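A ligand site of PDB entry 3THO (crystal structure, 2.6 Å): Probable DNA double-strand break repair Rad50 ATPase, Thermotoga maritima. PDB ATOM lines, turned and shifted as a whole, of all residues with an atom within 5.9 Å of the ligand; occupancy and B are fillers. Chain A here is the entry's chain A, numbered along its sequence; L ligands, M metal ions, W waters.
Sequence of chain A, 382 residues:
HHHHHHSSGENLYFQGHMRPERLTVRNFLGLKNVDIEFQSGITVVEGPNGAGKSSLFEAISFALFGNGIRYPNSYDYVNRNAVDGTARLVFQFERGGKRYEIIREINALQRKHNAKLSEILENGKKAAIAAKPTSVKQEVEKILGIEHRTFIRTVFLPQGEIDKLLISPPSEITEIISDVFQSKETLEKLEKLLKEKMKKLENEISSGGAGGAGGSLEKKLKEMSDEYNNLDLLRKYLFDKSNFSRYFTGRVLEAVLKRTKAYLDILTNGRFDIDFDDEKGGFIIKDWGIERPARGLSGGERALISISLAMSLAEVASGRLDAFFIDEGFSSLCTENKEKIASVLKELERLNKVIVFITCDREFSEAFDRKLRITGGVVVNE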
ATOM      1  N   LEU A  29      -8.708  18.292 -17.517  1.00  0.00           N
ATOM      2  CA  LEU A  29      -9.338  18.331 -16.195  1.00  0.00           C
ATOM      3  C   LEU A  29      -8.286  18.448 -15.083  1.00  0.00           C
ATOM      4  O   LEU A  29      -7.564  19.447 -15.027  1.00  0.00           O
ATOM      5  CB  LEU A  29     -10.264  17.132 -15.968  1.00  0.00           C
ATOM      6  CG  LEU A  29     -11.521  17.179 -16.851  1.00  0.00           C
ATOM      7  CD1 LEU A  29     -12.436  15.947 -16.611  1.00  0.00           C
ATOM      8  CD2 LEU A  29     -12.303  18.470 -16.601  1.00  0.00           C
ATOM      9  N   GLY A  30      -8.209  17.438 -14.217  1.00  0.00           N
ATOM     10  CA  GLY A  30      -7.274  17.431 -13.103  1.00  0.00           C
ATOM     11  C   GLY A  30      -5.996  16.657 -13.398  1.00  0.00           C
ATOM     12  O   GLY A  30      -5.121  16.535 -12.546  1.00  0.00           O
ATOM     13  N   LEU A  31      -5.893  16.131 -14.617  1.00  0.00           N
ATOM     14  CA  LEU A  31      -4.699  15.400 -15.040  1.00  0.00           C
ATOM     15  C   LEU A  31      -3.665  16.338 -15.681  1.00  0.00           C
ATOM     16  O   LEU A  31      -4.029  17.259 -16.425  1.00  0.00           O
ATOM     17  CB  LEU A  31      -5.072  14.304 -16.037  1.00  0.00           C
ATOM     18  CG  LEU A  31      -5.860  13.129 -15.435  1.00  0.00           C
ATOM     19  CD1 LEU A  31      -6.377  12.214 -16.537  1.00  0.00           C
ATOM     20  CD2 LEU A  31      -4.951  12.384 -14.460  1.00  0.00           C
ATOM     21  N   GLY A  47      -6.037   6.584  -5.413  1.00  0.00           N
ATOM     22  CA  GLY A  47      -5.446   7.872  -5.099  1.00  0.00           C
ATOM     23  C   GLY A  47      -6.445   8.754  -4.354  1.00  0.00           C
ATOM     24  O   GLY A  47      -7.622   8.425  -4.270  1.00  0.00           O
ATOM     25  N   PRO A  48      -5.962   9.878  -3.822  1.00  0.00           N
ATOM     26  CA  PRO A  48      -6.766  10.813  -3.019  1.00  0.00           C
ATOM     27  C   PRO A  48      -7.853  11.531  -3.845  1.00  0.00           C
ATOM     28  O   PRO A  48      -7.746  11.557  -5.062  1.00  0.00           O
ATOM     29  CB  PRO A  48      -5.731  11.864  -2.545  1.00  0.00           C
ATOM     30  CG  PRO A  48      -4.389  11.390  -3.020  1.00  0.00           C
ATOM     31  CD  PRO A  48      -4.599  10.366  -4.098  1.00  0.00           C
ATOM     32  N   ASN A  49      -8.860  12.107  -3.177  1.00  0.00           N
ATOM     33  CA  ASN A  49      -9.857  12.923  -3.858  1.00  0.00           C
ATOM     34  C   ASN A  49      -9.206  13.989  -4.730  1.00  0.00           C
ATOM     35  O   ASN A  49      -8.195  14.566  -4.344  1.00  0.00           O
ATOM     36  CB  ASN A  49     -10.769  13.640  -2.844  1.00  0.00           C
ATOM     37  CG  ASN A  49     -11.579  12.675  -2.001  1.00  0.00           C
ATOM     38  OD1 ASN A  49     -11.976  11.591  -2.465  1.00  0.00           O
ATOM     39  ND2 ASN A  49     -11.836  13.055  -0.754  1.00  0.00           N
ATOM     40  N   GLY A  50      -9.796  14.243  -5.910  1.00  0.00           N
ATOM     41  CA  GLY A  50      -9.299  15.283  -6.797  1.00  0.00           C
ATOM     42  C   GLY A  50      -7.918  14.967  -7.366  1.00  0.00           C
ATOM     43  O   GLY A  50      -7.286  15.826  -7.951  1.00  0.00           O
ATOM     44  N   ALA A  51      -7.458  13.734  -7.184  1.00  0.00           N
ATOM     45  CA  ALA A  51      -6.197  13.329  -7.771  1.00  0.00           C
ATOM     46  C   ALA A  51      -6.281  13.237  -9.308  1.00  0.00           C
ATOM     47  O   ALA A  51      -5.292  13.432 -10.017  1.00  0.00           O
ATOM     48  CB  ALA A  51      -5.720  12.009  -7.178  1.00  0.00           C
ATOM     49  N   GLY A  52      -7.472  12.946  -9.828  1.00  0.00           N
ATOM     50  CA  GLY A  52      -7.651  12.919 -11.272  1.00  0.00           C
ATOM     51  C   GLY A  52      -8.061  11.536 -11.767  1.00  0.00           C
ATOM     52  O   GLY A  52      -7.962  11.238 -12.973  1.00  0.00           O
ATOM     53  N   LYS A  53      -8.500  10.707 -10.833  1.00  0.00           N
ATOM     54  CA  LYS A  53      -8.962   9.365 -11.149  1.00  0.00           C
ATOM     55  C   LYS A  53     -10.144   9.414 -12.134  1.00  0.00           C
ATOM     56  O   LYS A  53     -10.089   8.881 -13.252  1.00  0.00           O
ATOM     57  CB  LYS A  53      -9.392   8.672  -9.861  1.00  0.00           C
ATOM     58  CG  LYS A  53      -8.309   7.813  -9.226  1.00  0.00           C
ATOM     59  CD  LYS A  53      -8.168   8.072  -7.727  1.00  0.00           C
ATOM     60  CE  LYS A  53      -9.525   8.281  -7.065  1.00  0.00           C
ATOM     61  NZ  LYS A  53      -9.477   9.468  -6.136  1.00  0.00           N
ATOM     62  N   SER A  54     -11.196  10.095 -11.743  1.00  0.00           N
ATOM     63  CA  SER A  54     -12.316  10.273 -12.664  1.00  0.00           C
ATOM     64  C   SER A  54     -11.916  10.960 -13.974  1.00  0.00           C
ATOM     65  O   SER A  54     -12.472  10.644 -15.041  1.00  0.00           O
ATOM     66  CB  SER A  54     -13.464  11.014 -11.978  1.00  0.00           C
ATOM     67  OG  SER A  54     -14.376  10.099 -11.424  1.00  0.00           O
ATOM     68  N   SER A  55     -10.975  11.890 -13.899  1.00  0.00           N
ATOM     69  CA  SER A  55     -10.505  12.636 -15.071  1.00  0.00           C
ATOM     70  C   SER A  55     -10.043  11.668 -16.141  1.00  0.00           C
ATOM     71  O   SER A  55     -10.314  11.847 -17.318  1.00  0.00           O
ATOM     72  CB  SER A  55      -9.354  13.561 -14.692  1.00  0.00           C
ATOM     73  OG  SER A  55      -9.792  14.539 -13.763  1.00  0.00           O
ATOM     74  N   LEU A  56      -9.330  10.653 -15.701  1.00  0.00           N
ATOM     75  CA  LEU A  56      -8.890   9.572 -16.560  1.00  0.00           C
ATOM     76  C   LEU A  56     -10.032   8.920 -17.352  1.00  0.00           C
ATOM     77  O   LEU A  56     -10.015   8.817 -18.585  1.00  0.00           O
ATOM     78  CB  LEU A  56      -8.282   8.515 -15.654  1.00  0.00           C
ATOM     79  CG  LEU A  56      -7.165   7.669 -16.198  1.00  0.00           C
ATOM     80  CD1 LEU A  56      -6.256   8.576 -17.030  1.00  0.00           C
ATOM     81  CD2 LEU A  56      -6.433   7.086 -14.978  1.00  0.00           C
ATOM     82  N   GLU A  58     -13.002  10.035 -17.809  1.00  0.00           N
ATOM     83  CA  GLU A  58     -13.614  11.006 -18.708  1.00  0.00           C
ATOM     84  C   GLU A  58     -12.787  11.198 -19.973  1.00  0.00           C
ATOM     85  O   GLU A  58     -13.339  11.295 -21.080  1.00  0.00           O
ATOM     86  CB  GLU A  58     -13.900  12.305 -17.975  1.00  0.00           C
ATOM     87  CG  GLU A  58     -14.783  12.081 -16.741  1.00  0.00           C
ATOM     88  CD  GLU A  58     -15.558  13.310 -16.273  1.00  0.00           C
ATOM     89  OE1 GLU A  58     -15.911  14.224 -17.086  1.00  0.00           O
ATOM     90  OE2 GLU A  58     -15.849  13.345 -15.052  1.00  0.00           O
ATOM     91  N   ARG A  70     -19.100  15.771 -17.517  1.00  0.00           N
ATOM     92  CA  ARG A  70     -19.040  16.749 -16.424  1.00  0.00           C
ATOM     93  C   ARG A  70     -19.204  18.223 -16.826  1.00  0.00           C
ATOM     94  O   ARG A  70     -19.689  19.036 -16.040  1.00  0.00           O
ATOM     95  CB  ARG A  70     -17.680  16.505 -15.745  1.00  0.00           C
ATOM     96  CG  ARG A  70     -17.281  17.447 -14.640  1.00  0.00           C
ATOM     97  CD  ARG A  70     -15.769  17.333 -14.430  1.00  0.00           C
ATOM     98  NE  ARG A  70     -15.296  15.958 -14.151  1.00  0.00           N
ATOM     99  CZ  ARG A  70     -14.550  15.616 -13.099  1.00  0.00           C
ATOM    100  NH1 ARG A  70     -14.184  16.534 -12.217  1.00  0.00           N
ATOM    101  NH2 ARG A  70     -14.137  14.355 -12.936  1.00  0.00           N
ATOM    102  N   TYR A  71     -18.751  18.585 -18.023  1.00  0.00           N
ATOM    103  CA  TYR A  71     -18.997  19.918 -18.581  1.00  0.00           C
ATOM    104  C   TYR A  71     -19.713  19.803 -19.939  1.00  0.00           C
ATOM    105  O   TYR A  71     -19.647  18.762 -20.593  1.00  0.00           O
ATOM    106  CB  TYR A  71     -17.686  20.687 -18.782  1.00  0.00           C
ATOM    107  CG  TYR A  71     -16.888  21.006 -17.529  1.00  0.00           C
ATOM    108  CD1 TYR A  71     -17.378  21.903 -16.569  1.00  0.00           C
ATOM    109  CD2 TYR A  71     -15.622  20.445 -17.317  1.00  0.00           C
ATOM    110  CE1 TYR A  71     -16.634  22.217 -15.429  1.00  0.00           C
ATOM    111  CE2 TYR A  71     -14.871  20.762 -16.184  1.00  0.00           C
ATOM    112  CZ  TYR A  71     -15.384  21.648 -15.239  1.00  0.00           C
ATOM    113  OH  TYR A  71     -14.656  21.955 -14.104  1.00  0.00           O
ATOM    114  N   TYR A  75     -13.935  23.334 -23.921  1.00  0.00           N
ATOM    115  CA  TYR A  75     -12.823  24.077 -23.348  1.00  0.00           C
ATOM    116  C   TYR A  75     -12.904  24.169 -21.827  1.00  0.00           C
ATOM    117  O   TYR A  75     -11.937  24.558 -21.160  1.00  0.00           O
ATOM    118  CB  TYR A  75     -12.716  25.451 -23.987  1.00  0.00           C
ATOM    119  CG  TYR A  75     -14.028  25.960 -24.529  1.00  0.00           C
ATOM    120  CD1 TYR A  75     -15.030  26.372 -23.670  1.00  0.00           C
ATOM    121  CD2 TYR A  75     -14.259  26.016 -25.902  1.00  0.00           C
ATOM    122  CE1 TYR A  75     -16.239  26.836 -24.143  1.00  0.00           C
ATOM    123  CE2 TYR A  75     -15.462  26.480 -26.399  1.00  0.00           C
ATOM    124  OH  TYR A  75     -17.662  27.370 -25.963  1.00  0.00           O
ATOM    125  N   ASP A  76     -14.051  23.792 -21.284  1.00  0.00           N
ATOM    126  CA  ASP A  76     -14.116  23.594 -19.854  1.00  0.00           C
ATOM    127  C   ASP A  76     -13.167  22.478 -19.405  1.00  0.00           C
ATOM    128  O   ASP A  76     -12.663  22.500 -18.286  1.00  0.00           O
ATOM    129  CB  ASP A  76     -15.563  23.347 -19.428  1.00  0.00           C
ATOM    130  CG  ASP A  76     -16.463  24.536 -19.757  1.00  0.00           C
ATOM    131  OD1 ASP A  76     -15.923  25.679 -19.755  1.00  0.00           O
ATOM    132  OD2 ASP A  76     -17.668  24.352 -20.041  1.00  0.00           O
ATOM    133  N   TYR A  77     -12.903  21.529 -20.300  1.00  0.00           N
ATOM    134  CA  TYR A  77     -12.070  20.381 -19.982  1.00  0.00           C
ATOM    135  C   TYR A  77     -10.582  20.707 -19.946  1.00  0.00           C
ATOM    136  O   TYR A  77      -9.779  19.883 -19.494  1.00  0.00           O
ATOM    137  CB  TYR A  77     -12.363  19.236 -20.956  1.00  0.00           C
ATOM    138  CG  TYR A  77     -13.729  18.684 -20.709  1.00  0.00           C
ATOM    139  CD1 TYR A  77     -13.924  17.607 -19.838  1.00  0.00           C
ATOM    140  CD2 TYR A  77     -14.845  19.281 -21.272  1.00  0.00           C
ATOM    141  CE1 TYR A  77     -15.180  17.124 -19.578  1.00  0.00           C
ATOM    142  CE2 TYR A  77     -16.121  18.804 -21.017  1.00  0.00           C
ATOM    143  CZ  TYR A  77     -16.282  17.725 -20.170  1.00  0.00           C
ATOM    144  OH  TYR A  77     -17.543  17.255 -19.910  1.00  0.00           O
ATOM    145  N   VAL A  78     -10.194  21.901 -20.416  1.00  0.00           N
ATOM    146  CA  VAL A  78      -8.773  22.262 -20.362  1.00  0.00           C
ATOM    147  C   VAL A  78      -8.345  22.438 -18.916  1.00  0.00           C
ATOM    148  O   VAL A  78      -9.052  23.091 -18.120  1.00  0.00           O
ATOM    149  CB  VAL A  78      -8.450  23.572 -21.145  1.00  0.00           C
ATOM    150  CG1 VAL A  78      -7.059  24.059 -20.786  1.00  0.00           C
ATOM    151  CG2 VAL A  78      -8.559  23.342 -22.642  1.00  0.00           C
ATOM    152  N   ASN A  79      -7.216  21.828 -18.550  1.00  0.00           N
ATOM    153  CA  ASN A  79      -6.675  22.015 -17.207  1.00  0.00           C
ATOM    154  C   ASN A  79      -6.304  23.485 -16.943  1.00  0.00           C
ATOM    155  O   ASN A  79      -5.222  23.981 -17.336  1.00  0.00           O
ATOM    156  CB  ASN A  79      -5.468  21.124 -16.982  1.00  0.00           C
ATOM    157  CG  ASN A  79      -4.996  21.149 -15.549  1.00  0.00           C
ATOM    158  OD1 ASN A  79      -5.261  22.127 -14.818  1.00  0.00           O
ATOM    159  ND2 ASN A  79      -4.305  20.085 -15.139  1.00  0.00           N
ATOM    160  N   ARG A  80      -7.208  24.181 -16.247  1.00  0.00           N
ATOM    161  CA  ARG A  80      -7.044  25.584 -15.917  1.00  0.00           C
ATOM    162  C   ARG A  80      -5.840  25.824 -15.005  1.00  0.00           C
ATOM    163  O   ARG A  80      -5.462  26.979 -14.789  1.00  0.00           O
ATOM    164  CB  ARG A  80      -8.309  26.100 -15.239  1.00  0.00           C
ATOM    165  CG  ARG A  80      -9.564  25.756 -15.985  1.00  0.00           C
ATOM    166  CD  ARG A  80      -9.603  26.435 -17.345  1.00  0.00           C
ATOM    167  NE  ARG A  80      -9.474  27.883 -17.197  1.00  0.00           N
ATOM    168  CZ  ARG A  80     -10.459  28.696 -16.847  1.00  0.00           C
ATOM    169  NH1 ARG A  80     -10.243  30.003 -16.721  1.00  0.00           N
ATOM    170  NH2 ARG A  80     -11.681  28.211 -16.611  1.00  0.00           N
ATOM    171  N   ASN A  81      -5.260  24.751 -14.457  1.00  0.00           N
ATOM    172  CA  ASN A  81      -4.111  24.899 -13.554  1.00  0.00           C
ATOM    173  C   ASN A  81      -2.787  24.560 -14.247  1.00  0.00           C
ATOM    174  O   ASN A  81      -1.782  24.282 -13.580  1.00  0.00           O
ATOM    175  CB  ASN A  81      -4.270  24.088 -12.257  1.00  0.00           C
ATOM    176  CG  ASN A  81      -5.413  24.612 -11.371  1.00  0.00           C
ATOM    177  OD1 ASN A  81      -5.596  25.814 -11.244  1.00  0.00           O
ATOM    178  ND2 ASN A  81      -6.166  23.696 -10.760  1.00  0.00           N
ATOM    179  N   ASP A 327     -16.427   3.653 -12.394  1.00  0.00           N
ATOM    180  CA  ASP A 327     -15.885   4.901 -11.867  1.00  0.00           C
ATOM    181  C   ASP A 327     -16.480   5.232 -10.492  1.00  0.00           C
ATOM    182  O   ASP A 327     -17.559   5.787 -10.393  1.00  0.00           O
ATOM    183  CB  ASP A 327     -16.179   6.029 -12.872  1.00  0.00           C
ATOM    184  CG  ASP A 327     -15.557   7.365 -12.452  1.00  0.00           C
ATOM    185  OD1 ASP A 327     -15.719   8.362 -13.216  1.00  0.00           O
ATOM    186  OD2 ASP A 327     -14.912   7.443 -11.384  1.00  0.00           O
ATOM    187  N   GLU A 328     -15.749   4.892  -9.439  1.00  0.00           N
ATOM    188  CA  GLU A 328     -16.130   5.229  -8.051  1.00  0.00           C
ATOM    189  C   GLU A 328     -17.538   4.745  -7.633  1.00  0.00           C
ATOM    190  O   GLU A 328     -18.214   5.411  -6.829  1.00  0.00           O
ATOM    191  CB  GLU A 328     -15.896   6.728  -7.742  1.00  0.00           C
ATOM    192  CG  GLU A 328     -14.938   7.450  -8.708  1.00  0.00           C
ATOM    193  CD  GLU A 328     -14.080   8.573  -8.075  1.00  0.00           C
ATOM    194  OE1 GLU A 328     -13.883   9.656  -8.703  1.00  0.00           O
ATOM    195  OE2 GLU A 328     -13.587   8.353  -6.945  1.00  0.00           O
ATOM    196  N   ILE A 358     -12.157   2.415 -10.513  1.00  0.00           N
ATOM    197  CA  ILE A 358     -11.638   3.608  -9.830  1.00  0.00           C
ATOM    198  C   ILE A 358     -12.215   3.696  -8.410  1.00  0.00           C
ATOM    199  O   ILE A 358     -13.424   3.734  -8.223  1.00  0.00           O
ATOM    200  CB  ILE A 358     -12.018   4.930 -10.549  1.00  0.00           C
ATOM    201  CG1 ILE A 358     -11.356   5.040 -11.929  1.00  0.00           C
ATOM    202  CG2 ILE A 358     -11.622   6.126  -9.705  1.00  0.00           C
ATOM    203  CD1 ILE A 358     -11.999   4.189 -13.007  1.00  0.00           C
HETATM  204  P1  LIG L   1     -10.897  12.074  -8.354  1.00  0.00           P
HETATM  205  O1  LIG L   1     -11.684  11.111  -9.250  1.00  0.00           O
HETATM  206  O2  LIG L   1      -9.415  11.611  -8.280  1.00  0.00           O
HETATM  207  O3  LIG L   1     -11.496  12.153  -6.933  1.00  0.00           O
HETATM  208  P2  LIG L   1     -11.385  14.114 -10.306  1.00  0.00           P
HETATM  209  O4  LIG L   1     -10.688  13.364 -11.425  1.00  0.00           O
HETATM  210  O5  LIG L   1     -12.924  14.081 -10.500  1.00  0.00           O
HETATM  211  O6  LIG L   1     -10.943  13.552  -8.872  1.00  0.00           O
HETATM  212  O7  LIG L   1     -11.029  15.634 -10.277  1.00  0.00           O
HETATM  213  C1  LIG L   1      -9.661  16.065 -10.382  1.00  0.00           C
HETATM  214  C2  LIG L   1      -9.378  17.460 -10.109  1.00  0.00           C
HETATM  215  O8  LIG L   1      -9.529  18.324 -11.298  1.00  0.00           O
HETATM  216  C3  LIG L   1     -10.303  18.034  -9.107  1.00  0.00           C
HETATM  217  O9  LIG L   1      -9.556  18.756  -8.234  1.00  0.00           O
HETATM  218  C4  LIG L   1     -11.219  18.894  -9.882  1.00  0.00           C
HETATM  219  O10 LIG L   1     -11.795  19.895  -9.168  1.00  0.00           O
HETATM  220  C5  LIG L   1     -10.284  19.457 -10.910  1.00  0.00           C
HETATM  221  N1  LIG L   1     -10.872  20.087 -12.071  1.00  0.00           N
HETATM  222  C6  LIG L   1     -12.159  20.022 -12.510  1.00  0.00           C
HETATM  223  N2  LIG L   1     -12.254  20.752 -13.629  1.00  0.00           N
HETATM  224  C7  LIG L   1     -11.028  21.283 -13.903  1.00  0.00           C
HETATM  225  C8  LIG L   1     -10.516  22.100 -14.931  1.00  0.00           C
HETATM  226  N3  LIG L   1     -11.318  22.555 -16.001  1.00  0.00           N
HETATM  227  N4  LIG L   1      -9.218  22.448 -14.883  1.00  0.00           N
HETATM  228  C9  LIG L   1      -8.401  22.018 -13.897  1.00  0.00           C
HETATM  229  N5  LIG L   1      -8.855  21.222 -12.918  1.00  0.00           N
HETATM  230  C10 LIG L   1     -10.153  20.855 -12.896  1.00  0.00           C
HETATM  231 MG    MG M   1     -14.462  12.416  -8.767  1.00  0.00          MG
HETATM  232  O   HOH W   1      -6.491  20.730 -11.292  1.00  0.00           O
HETATM  233  O   HOH W   2     -11.676   9.820  -4.990  1.00  0.00           O
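The backbone carbonyl oxygen of Asp 76 sits at hydrogen-bond distance from a nitrogen (N3) of the ligand, at 2.7 Å. An oxygen (O1) of the ligand lies close to the side-chain carboxylate of Glu 328, 2.7 Å away. The side-chain hydroxyl of Tyr 71 lies within hydrogen-bond range of a nitrogen (N2) of the ligand, 2.7 Å away. NH2 of Arg 70 lies within salt-bridge range of O5 of the ligand, at 2.7 Å. N of Ser 54 lies within hydrogen-bond range of O1 of the ligand (2.7 Å). An oxygen (O4) of the ligand lies within hydrogen-bond range of the backbone NH (N) of Ser 55. OG of Ser 55 lies within hydrogen-bond range of O4 of the ligand (2.8 Å). The backbone NH (N) of Gly 52 lies within hydrogen-bond range of an oxygen (O2) of the ligand (2.8 Å). The backbone NH (N) of Lys 53 sits at hydrogen-bond distance from an oxygen (O2) of the ligand. NZ of Lys 53 lies within salt-bridge range of O2 of the ligand, 3.0 Å away. N of Gly 50 lies within hydrogen-bond range of O3 of the ligand. A nitrogen (N4) of the ligand lies within hydrogen-bond range of the backbone NH (N) of Arg 80 (3.0 Å). O8 of the ligand lies close to N of Gly 30, at 3.3 Å. N of Ala 51 lies within hydrogen-bond range of O2 of the ligand, at 3.1 Å. The backbone carbonyl oxygen (O) of Val 78 lies within hydrogen-bond range of a nitrogen (N3) of the ligand, at 3.1 Å.
The side-chain hydroxyl (OG) of Ser 54 sits at hydrogen-bond distance from the side-chain carboxylate (OE1) of Glu 328 (2.8 Å). N of Glu 328 sits at hydrogen-bond distance from O of Ile 358 (2.9 Å). The side-chain hydroxyl (OH) of Tyr 77 lies within hydrogen-bond range of the backbone NH (N) of Arg 70, at 3.2 Å. OG of Ser 54 lies within hydrogen-bond range of OD2 of Asp 327 (2.7 Å). The side-chain hydroxyl (OG) of Ser 55 sits at hydrogen-bond distance from the backbone NH (N) of Gly 30 (3.3 Å). The backbone carbonyl oxygen (O) of Pro 48 lies within hydrogen-bond range of the side-chain amino group (NZ) of Lys 53 (2.9 Å). The side-chain amino group (NZ) of Lys 53 is in hydrogen-bond range of the backbone carbonyl oxygen (O) of Gly 47 (2.8 Å). OD1 of Asn 79 is in hydrogen-bond range of N of Asn 81, at 2.6 Å.
N5 of the ligand sits close to O of Leu 29, at 3.0 Å. Residues that only touch the ligand: Pro 48, Asn 49 and Asn 79. 17 residues have an atom within 4 Å of the ligand: Leu 29, Gly 30, Pro 48, Asn 49, Gly 50, Ala 51, Gly 52, Lys 53, Ser 54, Ser 55, Arg 70, Tyr 71, Asp 76, Val 78, Asn 79, Arg 80 and Glu 328.
Water W1 bridges a nitrogen (N5) of the ligand (2.9 Å) and the side-chain amide nitrogen of Asn 81 (3.0 Å). Water W2 lies within hydrogen-bond range of NZ of Lys 53, O3 of the ligand, OD1 of Asn 49 and OE2 of Glu 328.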
